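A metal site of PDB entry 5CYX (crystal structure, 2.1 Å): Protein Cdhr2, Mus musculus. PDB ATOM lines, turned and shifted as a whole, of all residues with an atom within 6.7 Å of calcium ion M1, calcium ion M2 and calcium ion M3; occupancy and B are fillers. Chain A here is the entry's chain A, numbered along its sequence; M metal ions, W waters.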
ATOM      1  N   GLU A  18     -17.302 -20.486  16.308  1.00  0.00           N
ATOM      2  CA  GLU A  18     -16.671 -20.928  17.538  1.00  0.00           C
ATOM      3  C   GLU A  18     -15.831 -22.207  17.359  1.00  0.00           C
ATOM      4  O   GLU A  18     -14.988 -22.458  18.124  1.00  0.00           O
ATOM      5  CB  GLU A  18     -17.713 -21.095  18.651  1.00  0.00           C
ATOM      6  CG  GLU A  18     -18.643 -22.308  18.585  1.00  0.00           C
ATOM      7  CD  GLU A  18     -19.317 -22.623  19.907  1.00  0.00           C
ATOM      8  OE1 GLU A  18     -18.681 -22.444  21.004  1.00  0.00           O
ATOM      9  OE2 GLU A  18     -20.482 -23.103  19.898  1.00  0.00           O
ATOM     10  N   LEU A  66     -12.107 -20.089  20.779  1.00  0.00           N
ATOM     11  CA  LEU A  66     -13.337 -19.379  20.839  1.00  0.00           C
ATOM     12  C   LEU A  66     -14.370 -20.289  21.461  1.00  0.00           C
ATOM     13  O   LEU A  66     -14.304 -21.503  21.268  1.00  0.00           O
ATOM     14  CB  LEU A  66     -13.824 -19.059  19.414  1.00  0.00           C
ATOM     15  CG  LEU A  66     -13.010 -18.080  18.591  1.00  0.00           C
ATOM     16  CD1 LEU A  66     -13.642 -17.894  17.217  1.00  0.00           C
ATOM     17  CD2 LEU A  66     -12.908 -16.730  19.277  1.00  0.00           C
ATOM     18  N   ASP A  67     -15.351 -19.696  22.140  1.00  0.00           N
ATOM     19  CA  ASP A  67     -16.354 -20.491  22.827  1.00  0.00           C
ATOM     20  C   ASP A  67     -17.581 -19.634  23.045  1.00  0.00           C
ATOM     21  O   ASP A  67     -17.619 -18.772  23.928  1.00  0.00           O
ATOM     22  CB  ASP A  67     -15.806 -21.017  24.205  1.00  0.00           C
ATOM     23  CG  ASP A  67     -16.819 -21.917  24.919  1.00  0.00           C
ATOM     24  OD1 ASP A  67     -17.784 -22.431  24.301  1.00  0.00           O
ATOM     25  OD2 ASP A  67     -16.704 -22.096  26.116  1.00  0.00           O
ATOM     26  N   PHE A  68     -18.591 -19.862  22.221  1.00  0.00           N
ATOM     27  CA  PHE A  68     -19.807 -19.127  22.267  1.00  0.00           C
ATOM     28  C   PHE A  68     -20.471 -19.226  23.625  1.00  0.00           C
ATOM     29  O   PHE A  68     -21.014 -18.247  24.111  1.00  0.00           O
ATOM     30  CB  PHE A  68     -20.793 -19.673  21.231  1.00  0.00           C
ATOM     31  CG  PHE A  68     -22.099 -18.963  21.242  1.00  0.00           C
ATOM     32  CD1 PHE A  68     -22.228 -17.727  20.632  1.00  0.00           C
ATOM     33  CD2 PHE A  68     -23.218 -19.515  21.872  1.00  0.00           C
ATOM     34  CE1 PHE A  68     -23.457 -17.074  20.617  1.00  0.00           C
ATOM     35  CE2 PHE A  68     -24.438 -18.865  21.867  1.00  0.00           C
ATOM     36  CZ  PHE A  68     -24.537 -17.640  21.265  1.00  0.00           C
ATOM     37  N   GLU A  69     -20.403 -20.408  24.237  1.00  0.00           N
ATOM     38  CA  GLU A  69     -21.072 -20.627  25.515  1.00  0.00           C
ATOM     39  C   GLU A  69     -20.558 -19.719  26.654  1.00  0.00           C
ATOM     40  O   GLU A  69     -21.341 -19.408  27.579  1.00  0.00           O
ATOM     41  CB  GLU A  69     -20.981 -22.094  25.935  1.00  0.00           C
ATOM     42  CG  GLU A  69     -21.998 -22.986  25.252  1.00  0.00           C
ATOM     43  CD  GLU A  69     -21.842 -23.073  23.723  1.00  0.00           C
ATOM     44  OE1 GLU A  69     -20.778 -23.358  23.178  1.00  0.00           O
ATOM     45  OE2 GLU A  69     -22.790 -22.845  23.017  1.00  0.00           O
ATOM     46  N   THR A  70     -19.301 -19.260  26.594  1.00  0.00           N
ATOM     47  CA  THR A  70     -18.746 -18.322  27.608  1.00  0.00           C
ATOM     48  C   THR A  70     -18.522 -16.897  27.117  1.00  0.00           C
ATOM     49  O   THR A  70     -18.821 -15.955  27.839  1.00  0.00           O
ATOM     50  CB  THR A  70     -17.418 -18.809  28.188  1.00  0.00           C
ATOM     51  OG1 THR A  70     -16.869 -19.764  27.285  1.00  0.00           O
ATOM     52  CG2 THR A  70     -17.597 -19.486  29.513  1.00  0.00           C
ATOM     53  N   GLU A  96     -19.990 -17.012  16.501  1.00  0.00           N
ATOM     54  CA  GLU A  96     -21.196 -17.782  16.171  1.00  0.00           C
ATOM     55  C   GLU A  96     -21.244 -19.152  16.851  1.00  0.00           C
ATOM     56  O   GLU A  96     -20.249 -19.925  16.868  1.00  0.00           O
ATOM     57  CB  GLU A  96     -21.314 -18.007  14.671  1.00  0.00           C
ATOM     58  CG  GLU A  96     -21.732 -16.796  13.876  1.00  0.00           C
ATOM     59  CD  GLU A  96     -22.157 -17.145  12.441  1.00  0.00           C
ATOM     60  OE1 GLU A  96     -21.567 -18.095  11.863  1.00  0.00           O
ATOM     61  OE2 GLU A  96     -23.069 -16.430  11.925  1.00  0.00           O
ATOM     62  N   ASP A  97     -22.436 -19.478  17.331  1.00  0.00           N
ATOM     63  CA  ASP A  97     -22.715 -20.743  17.978  1.00  0.00           C
ATOM     64  C   ASP A  97     -22.553 -21.879  16.962  1.00  0.00           C
ATOM     65  O   ASP A  97     -22.972 -21.743  15.782  1.00  0.00           O
ATOM     66  CB  ASP A  97     -24.159 -20.761  18.553  1.00  0.00           C
ATOM     67  CG  ASP A  97     -24.391 -21.944  19.522  1.00  0.00           C
ATOM     68  OD1 ASP A  97     -23.408 -22.509  20.078  1.00  0.00           O
ATOM     69  OD2 ASP A  97     -25.579 -22.345  19.675  1.00  0.00           O
ATOM     70  N   ARG A  98     -21.910 -22.962  17.408  1.00  0.00           N
ATOM     71  CA  ARG A  98     -21.930 -24.248  16.616  1.00  0.00           C
ATOM     72  C   ARG A  98     -22.331 -25.407  17.561  1.00  0.00           C
ATOM     73  O   ARG A  98     -22.249 -25.289  18.837  1.00  0.00           O
ATOM     74  CB  ARG A  98     -20.585 -24.472  15.973  1.00  0.00           C
ATOM     75  CG  ARG A  98     -20.208 -23.464  14.899  1.00  0.00           C
ATOM     76  CD  ARG A  98     -20.841 -23.865  13.597  1.00  0.00           C
ATOM     77  NE  ARG A  98     -20.606 -22.912  12.527  1.00  0.00           N
ATOM     78  CZ  ARG A  98     -21.306 -21.818  12.282  1.00  0.00           C
ATOM     79  NH1 ARG A  98     -20.989 -21.060  11.256  1.00  0.00           N
ATOM     80  NH2 ARG A  98     -22.331 -21.453  13.040  1.00  0.00           N
ATOM     81  N   ASN A  99     -22.805 -26.507  16.981  1.00  0.00           N
ATOM     82  CA  ASN A  99     -23.272 -27.618  17.775  1.00  0.00           C
ATOM     83  C   ASN A  99     -22.117 -28.481  18.331  1.00  0.00           C
ATOM     84  O   ASN A  99     -21.852 -29.600  17.820  1.00  0.00           O
ATOM     85  CB  ASN A  99     -24.253 -28.475  17.012  1.00  0.00           C
ATOM     86  CG  ASN A  99     -25.017 -29.397  17.875  1.00  0.00           C
ATOM     87  OD1 ASN A  99     -24.955 -29.309  19.101  1.00  0.00           O
ATOM     88  ND2 ASN A  99     -25.714 -30.299  17.262  1.00  0.00           N
ATOM     89  N   ASP A 100     -21.452 -27.944  19.362  1.00  0.00           N
ATOM     90  CA  ASP A 100     -20.350 -28.648  20.051  1.00  0.00           C
ATOM     91  C   ASP A 100     -20.774 -29.101  21.439  1.00  0.00           C
ATOM     92  O   ASP A 100     -19.942 -29.568  22.169  1.00  0.00           O
ATOM     93  CB  ASP A 100     -19.116 -27.733  20.185  1.00  0.00           C
ATOM     94  CG  ASP A 100     -19.443 -26.385  20.935  1.00  0.00           C
ATOM     95  OD1 ASP A 100     -20.618 -26.028  21.105  1.00  0.00           O
ATOM     96  OD2 ASP A 100     -18.529 -25.698  21.386  1.00  0.00           O
ATOM     97  N   ASN A 101     -22.045 -28.917  21.868  1.00  0.00           N
ATOM     98  CA  ASN A 101     -22.414 -29.531  23.169  1.00  0.00           C
ATOM     99  C   ASN A 101     -23.424 -30.657  23.005  1.00  0.00           C
ATOM    100  O   ASN A 101     -24.181 -30.648  22.023  1.00  0.00           O
ATOM    101  CB  ASN A 101     -22.891 -28.510  24.181  1.00  0.00           C
ATOM    102  CG  ASN A 101     -21.766 -27.668  24.713  1.00  0.00           C
ATOM    103  OD1 ASN A 101     -20.984 -28.118  25.571  1.00  0.00           O
ATOM    104  ND2 ASN A 101     -21.646 -26.461  24.221  1.00  0.00           N
ATOM    105  N   ILE A 102     -23.359 -31.637  23.932  1.00  0.00           N
ATOM    106  CA  ILE A 102     -24.350 -32.727  24.006  1.00  0.00           C
ATOM    107  C   ILE A 102     -25.433 -32.525  25.099  1.00  0.00           C
ATOM    108  O   ILE A 102     -25.209 -31.818  26.109  1.00  0.00           O
ATOM    109  CB  ILE A 102     -23.735 -34.115  24.202  1.00  0.00           C
ATOM    110  CG1 ILE A 102     -23.004 -34.229  25.575  1.00  0.00           C
ATOM    111  CG2 ILE A 102     -22.713 -34.447  23.115  1.00  0.00           C
ATOM    112  CD1 ILE A 102     -22.522 -35.650  25.841  1.00  0.00           C
ATOM    113  N   PRO A 103     -26.585 -33.198  24.915  1.00  0.00           N
ATOM    114  CA  PRO A 103     -27.583 -33.250  25.954  1.00  0.00           C
ATOM    115  C   PRO A 103     -27.066 -34.046  27.124  1.00  0.00           C
ATOM    116  O   PRO A 103     -26.569 -35.141  26.937  1.00  0.00           O
ATOM    117  CB  PRO A 103     -28.726 -34.010  25.278  1.00  0.00           C
ATOM    118  CG  PRO A 103     -28.593 -33.689  23.831  1.00  0.00           C
ATOM    119  CD  PRO A 103     -27.099 -33.732  23.642  1.00  0.00           C
ATOM    120  N   ASP A 131     -28.938 -29.166  27.055  1.00  0.00           N
ATOM    121  CA  ASP A 131     -27.895 -29.033  26.058  1.00  0.00           C
ATOM    122  C   ASP A 131     -27.575 -27.569  25.998  1.00  0.00           C
ATOM    123  O   ASP A 131     -28.452 -26.760  25.710  1.00  0.00           O
ATOM    124  CB  ASP A 131     -28.403 -29.534  24.702  1.00  0.00           C
ATOM    125  CG  ASP A 131     -27.338 -29.510  23.613  1.00  0.00           C
ATOM    126  OD1 ASP A 131     -26.627 -28.511  23.415  1.00  0.00           O
ATOM    127  OD2 ASP A 131     -27.250 -30.500  22.842  1.00  0.00           O
ATOM    128  N   LYS A 132     -26.314 -27.233  26.237  1.00  0.00           N
ATOM    129  CA  LYS A 132     -25.901 -25.826  26.359  1.00  0.00           C
ATOM    130  C   LYS A 132     -25.895 -25.001  25.078  1.00  0.00           C
ATOM    131  O   LYS A 132     -25.796 -23.787  25.162  1.00  0.00           O
ATOM    132  CB  LYS A 132     -24.536 -25.750  27.003  1.00  0.00           C
ATOM    133  CG  LYS A 132     -24.585 -26.261  28.436  1.00  0.00           C
ATOM    134  CD  LYS A 132     -23.918 -25.282  29.381  1.00  0.00           C
ATOM    135  CE  LYS A 132     -22.403 -25.354  29.301  1.00  0.00           C
ATOM    136  NZ  LYS A 132     -21.747 -24.027  29.599  1.00  0.00           N
ATOM    137  N   ASP A 133     -26.024 -25.630  23.908  1.00  0.00           N
ATOM    138  CA  ASP A 133     -26.025 -24.856  22.686  1.00  0.00           C
ATOM    139  C   ASP A 133     -27.375 -24.107  22.612  1.00  0.00           C
ATOM    140  O   ASP A 133     -28.276 -24.354  23.399  1.00  0.00           O
ATOM    141  CB  ASP A 133     -25.769 -25.729  21.438  1.00  0.00           C
ATOM    142  CG  ASP A 133     -24.442 -26.507  21.552  1.00  0.00           C
ATOM    143  OD1 ASP A 133     -23.412 -25.877  21.921  1.00  0.00           O
ATOM    144  OD2 ASP A 133     -24.521 -27.715  21.393  1.00  0.00           O
ATOM    145  N   THR A 134     -27.456 -23.193  21.640  1.00  0.00           N
ATOM    146  CA  THR A 134     -28.622 -22.329  21.435  1.00  0.00           C
ATOM    147  C   THR A 134     -29.261 -22.661  20.081  1.00  0.00           C
ATOM    148  O   THR A 134     -28.572 -23.067  19.156  1.00  0.00           O
ATOM    149  CB  THR A 134     -28.145 -20.871  21.427  1.00  0.00           C
ATOM    150  OG1 THR A 134     -27.592 -20.535  22.722  1.00  0.00           O
ATOM    151  CG2 THR A 134     -29.332 -19.877  21.114  1.00  0.00           C
ATOM    152  N   THR A 136     -31.645 -24.863  17.417  1.00  0.00           N
ATOM    153  CA  THR A 136     -31.975 -26.289  17.284  1.00  0.00           C
ATOM    154  C   THR A 136     -30.823 -27.118  17.813  1.00  0.00           C
ATOM    155  O   THR A 136     -31.021 -28.251  18.213  1.00  0.00           O
ATOM    156  CB  THR A 136     -32.298 -26.708  15.844  1.00  0.00           C
ATOM    157  OG1 THR A 136     -31.175 -26.430  15.032  1.00  0.00           O
ATOM    158  CG2 THR A 136     -33.538 -25.855  15.303  1.00  0.00           C
ATOM    159  N   ALA A 137     -29.622 -26.578  17.798  1.00  0.00           N
ATOM    160  CA  ALA A 137     -28.488 -27.282  18.400  1.00  0.00           C
ATOM    161  C   ALA A 137     -28.645 -27.477  19.887  1.00  0.00           C
ATOM    162  O   ALA A 137     -27.897 -28.277  20.517  1.00  0.00           O
ATOM    163  CB  ALA A 137     -27.221 -26.510  18.140  1.00  0.00           C
ATOM    164  N   GLY A 138     -29.536 -26.677  20.507  1.00  0.00           N
ATOM    165  CA  GLY A 138     -29.812 -26.791  21.920  1.00  0.00           C
ATOM    166  C   GLY A 138     -31.125 -27.443  22.295  1.00  0.00           C
ATOM    167  O   GLY A 138     -31.417 -27.608  23.454  1.00  0.00           O
ATOM    168  N   LEU A 139     -31.907 -27.846  21.312  1.00  0.00           N
ATOM    169  CA  LEU A 139     -33.291 -28.222  21.492  1.00  0.00           C
ATOM    170  C   LEU A 139     -33.332 -29.756  21.592  1.00  0.00           C
ATOM    171  O   LEU A 139     -33.083 -30.493  20.566  1.00  0.00           O
ATOM    172  CB  LEU A 139     -34.090 -27.758  20.283  1.00  0.00           C
ATOM    173  CG  LEU A 139     -35.611 -27.889  20.377  1.00  0.00           C
ATOM    174  CD1 LEU A 139     -36.136 -27.120  21.592  1.00  0.00           C
ATOM    175  CD2 LEU A 139     -36.243 -27.344  19.101  1.00  0.00           C
ATOM    176  N   ASP A 189     -30.004 -33.599  20.403  1.00  0.00           N
ATOM    177  CA  ASP A 189     -30.450 -32.289  20.042  1.00  0.00           C
ATOM    178  C   ASP A 189     -31.145 -32.425  18.660  1.00  0.00           C
ATOM    179  O   ASP A 189     -31.190 -33.530  18.052  1.00  0.00           O
ATOM    180  CB  ASP A 189     -29.322 -31.235  20.108  1.00  0.00           C
ATOM    181  CG  ASP A 189     -28.125 -31.574  19.261  1.00  0.00           C
ATOM    182  OD1 ASP A 189     -28.310 -32.168  18.190  1.00  0.00           O
ATOM    183  OD2 ASP A 189     -26.970 -31.292  19.698  1.00  0.00           O
ATOM    184  N   SER A 190     -31.589 -31.313  18.151  1.00  0.00           N
ATOM    185  CA  SER A 190     -32.374 -31.253  16.917  1.00  0.00           C
ATOM    186  C   SER A 190     -31.467 -30.805  15.746  1.00  0.00           C
ATOM    187  O   SER A 190     -31.918 -30.386  14.718  1.00  0.00           O
ATOM    188  CB  SER A 190     -33.566 -30.292  17.125  1.00  0.00           C
ATOM    189  OG  SER A 190     -34.355 -30.630  18.262  1.00  0.00           O
ATOM    190  N   THR A 200     -25.714 -33.618  14.587  1.00  0.00           N
ATOM    191  CA  THR A 200     -26.680 -33.842  15.673  1.00  0.00           C
ATOM    192  C   THR A 200     -25.899 -34.484  16.797  1.00  0.00           C
ATOM    193  O   THR A 200     -25.116 -35.396  16.524  1.00  0.00           O
ATOM    194  CB  THR A 200     -27.803 -34.795  15.224  1.00  0.00           C
ATOM    195  OG1 THR A 200     -28.613 -34.163  14.202  1.00  0.00           O
ATOM    196  CG2 THR A 200     -28.673 -35.216  16.418  1.00  0.00           C
ATOM    197  N   GLN A 201     -26.088 -34.044  18.042  1.00  0.00           N
ATOM    198  CA  GLN A 201     -25.362 -34.694  19.183  1.00  0.00           C
ATOM    199  C   GLN A 201     -26.300 -35.506  20.041  1.00  0.00           C
ATOM    200  O   GLN A 201     -27.458 -35.097  20.240  1.00  0.00           O
ATOM    201  CB  GLN A 201     -24.673 -33.653  20.040  1.00  0.00           C
ATOM    202  CG  GLN A 201     -23.705 -32.760  19.295  1.00  0.00           C
ATOM    203  CD  GLN A 201     -22.296 -33.307  19.229  1.00  0.00           C
ATOM    204  OE1 GLN A 201     -22.039 -34.441  19.627  1.00  0.00           O
ATOM    205  NE2 GLN A 201     -21.388 -32.495  18.739  1.00  0.00           N
HETATM  206 CA    CA M   1     -22.062 -24.167  20.997  1.00  0.00          CA
HETATM  207 CA    CA M   2     -18.478 -24.020  22.782  1.00  0.00          CA
HETATM  208 CA    CA M   3     -26.006 -29.503  21.150  1.00  0.00          CA
HETATM  209  O   HOH W   1     -18.482 -25.769  24.509  1.00  0.00           O
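Within 4 Å of calcium ion M3: Asn 99, Asn 101, Asp 131, Asp 133, Ala 137 and Asp 189. The nearest printed residue that does not touch calcium ion M3 is Ile 102 (4.4 Å).
Calcium ion M3 is bound by OD1 of Asn 99, at 2.3 Å. The side-chain carboxylate (OD2) of Asp 131 is bound to calcium ion M3. Calcium ion M3 is bound by O of Asn 101 (2.3 Å). Calcium ion M3 is bound by the side-chain carboxylate (OD2) of Asp 133 (2.3 Å). Calcium ion M3 is bound by O of Ala 137, 2.3 Å away. The side-chain carboxylate (OD2) of Asp 189 binds calcium ion M3, 2.5 Å away. The side-chain carboxylate (OD1) of Asp 131 is bound to calcium ion M3.
Of the 26 residues printed, 7 come within 4 Å of calcium ion M1. The nearest printed residue that does not touch calcium ion M1 is Phe 68 (4.7 Å).
The side-chain amide nitrogen (ND2) of Asn 101 lies close to the side-chain carboxylate (OD1) of Asp 100, at 3.3 Å. N of Phe 68 lies close to OE1 of Glu 18 (2.9 Å). The backbone NH of Glu 18 lies within hydrogen-bond range of the backbone carbonyl oxygen of Glu 96 (3.1 Å). The side-chain carboxylate of Asp 67 lies within hydrogen-bond range of the side-chain hydroxyl of Thr 70. The side-chain amide nitrogen (ND2) of Asn 101 lies close to the side-chain carboxylate (OE1) of Glu 69 (3.4 Å). The side-chain carboxylate (OD2) of Asp 97 is in hydrogen-bond range of the backbone NH (N) of Thr 134 (2.8 Å). The side-chain carboxylate of Glu 96 lies within salt-bridge range of the guanidinium group of Arg 98 (3.1 Å). OD1 of Asp 189 is in hydrogen-bond range of N of Gln 201 (2.9 Å).
Calcium ion M1 is bound by the side-chain carboxylate (OE2) of Glu 18 (2.2 Å), the side-chain carboxylate (OD1) of Asp 97 (2.3 Å), the side-chain carboxylate (OD1) of Asp 100 (2.4 Å), the side-chain carboxylate (OD1) of Asp 133 (2.4 Å), the backbone carbonyl oxygen (O) of Arg 98 (2.4 Å), the side-chain carboxylate (OE2) of Glu 69 (2.5 Å) and the side-chain carboxylate (OE1) of Glu 69 (2.7 Å).
Calcium ion M2 is bound by the side-chain carboxylate (OD2) of Asp 100, 2.2 Å away. The side-chain carboxylate (OD1) of Asp 67 is bound to calcium ion M2 (2.3 Å). OE1 of Glu 18 binds calcium ion M2, at 2.4 Å. Calcium ion M2 is bound by the side-chain carboxylate (OE1) of Glu 69. Calcium ion M2 is bound by water W1 (2.5 Å).
Four residues have an atom within 4 Å of calcium ion M2: Glu 18, Asp 67, Glu 69 and Asp 100.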
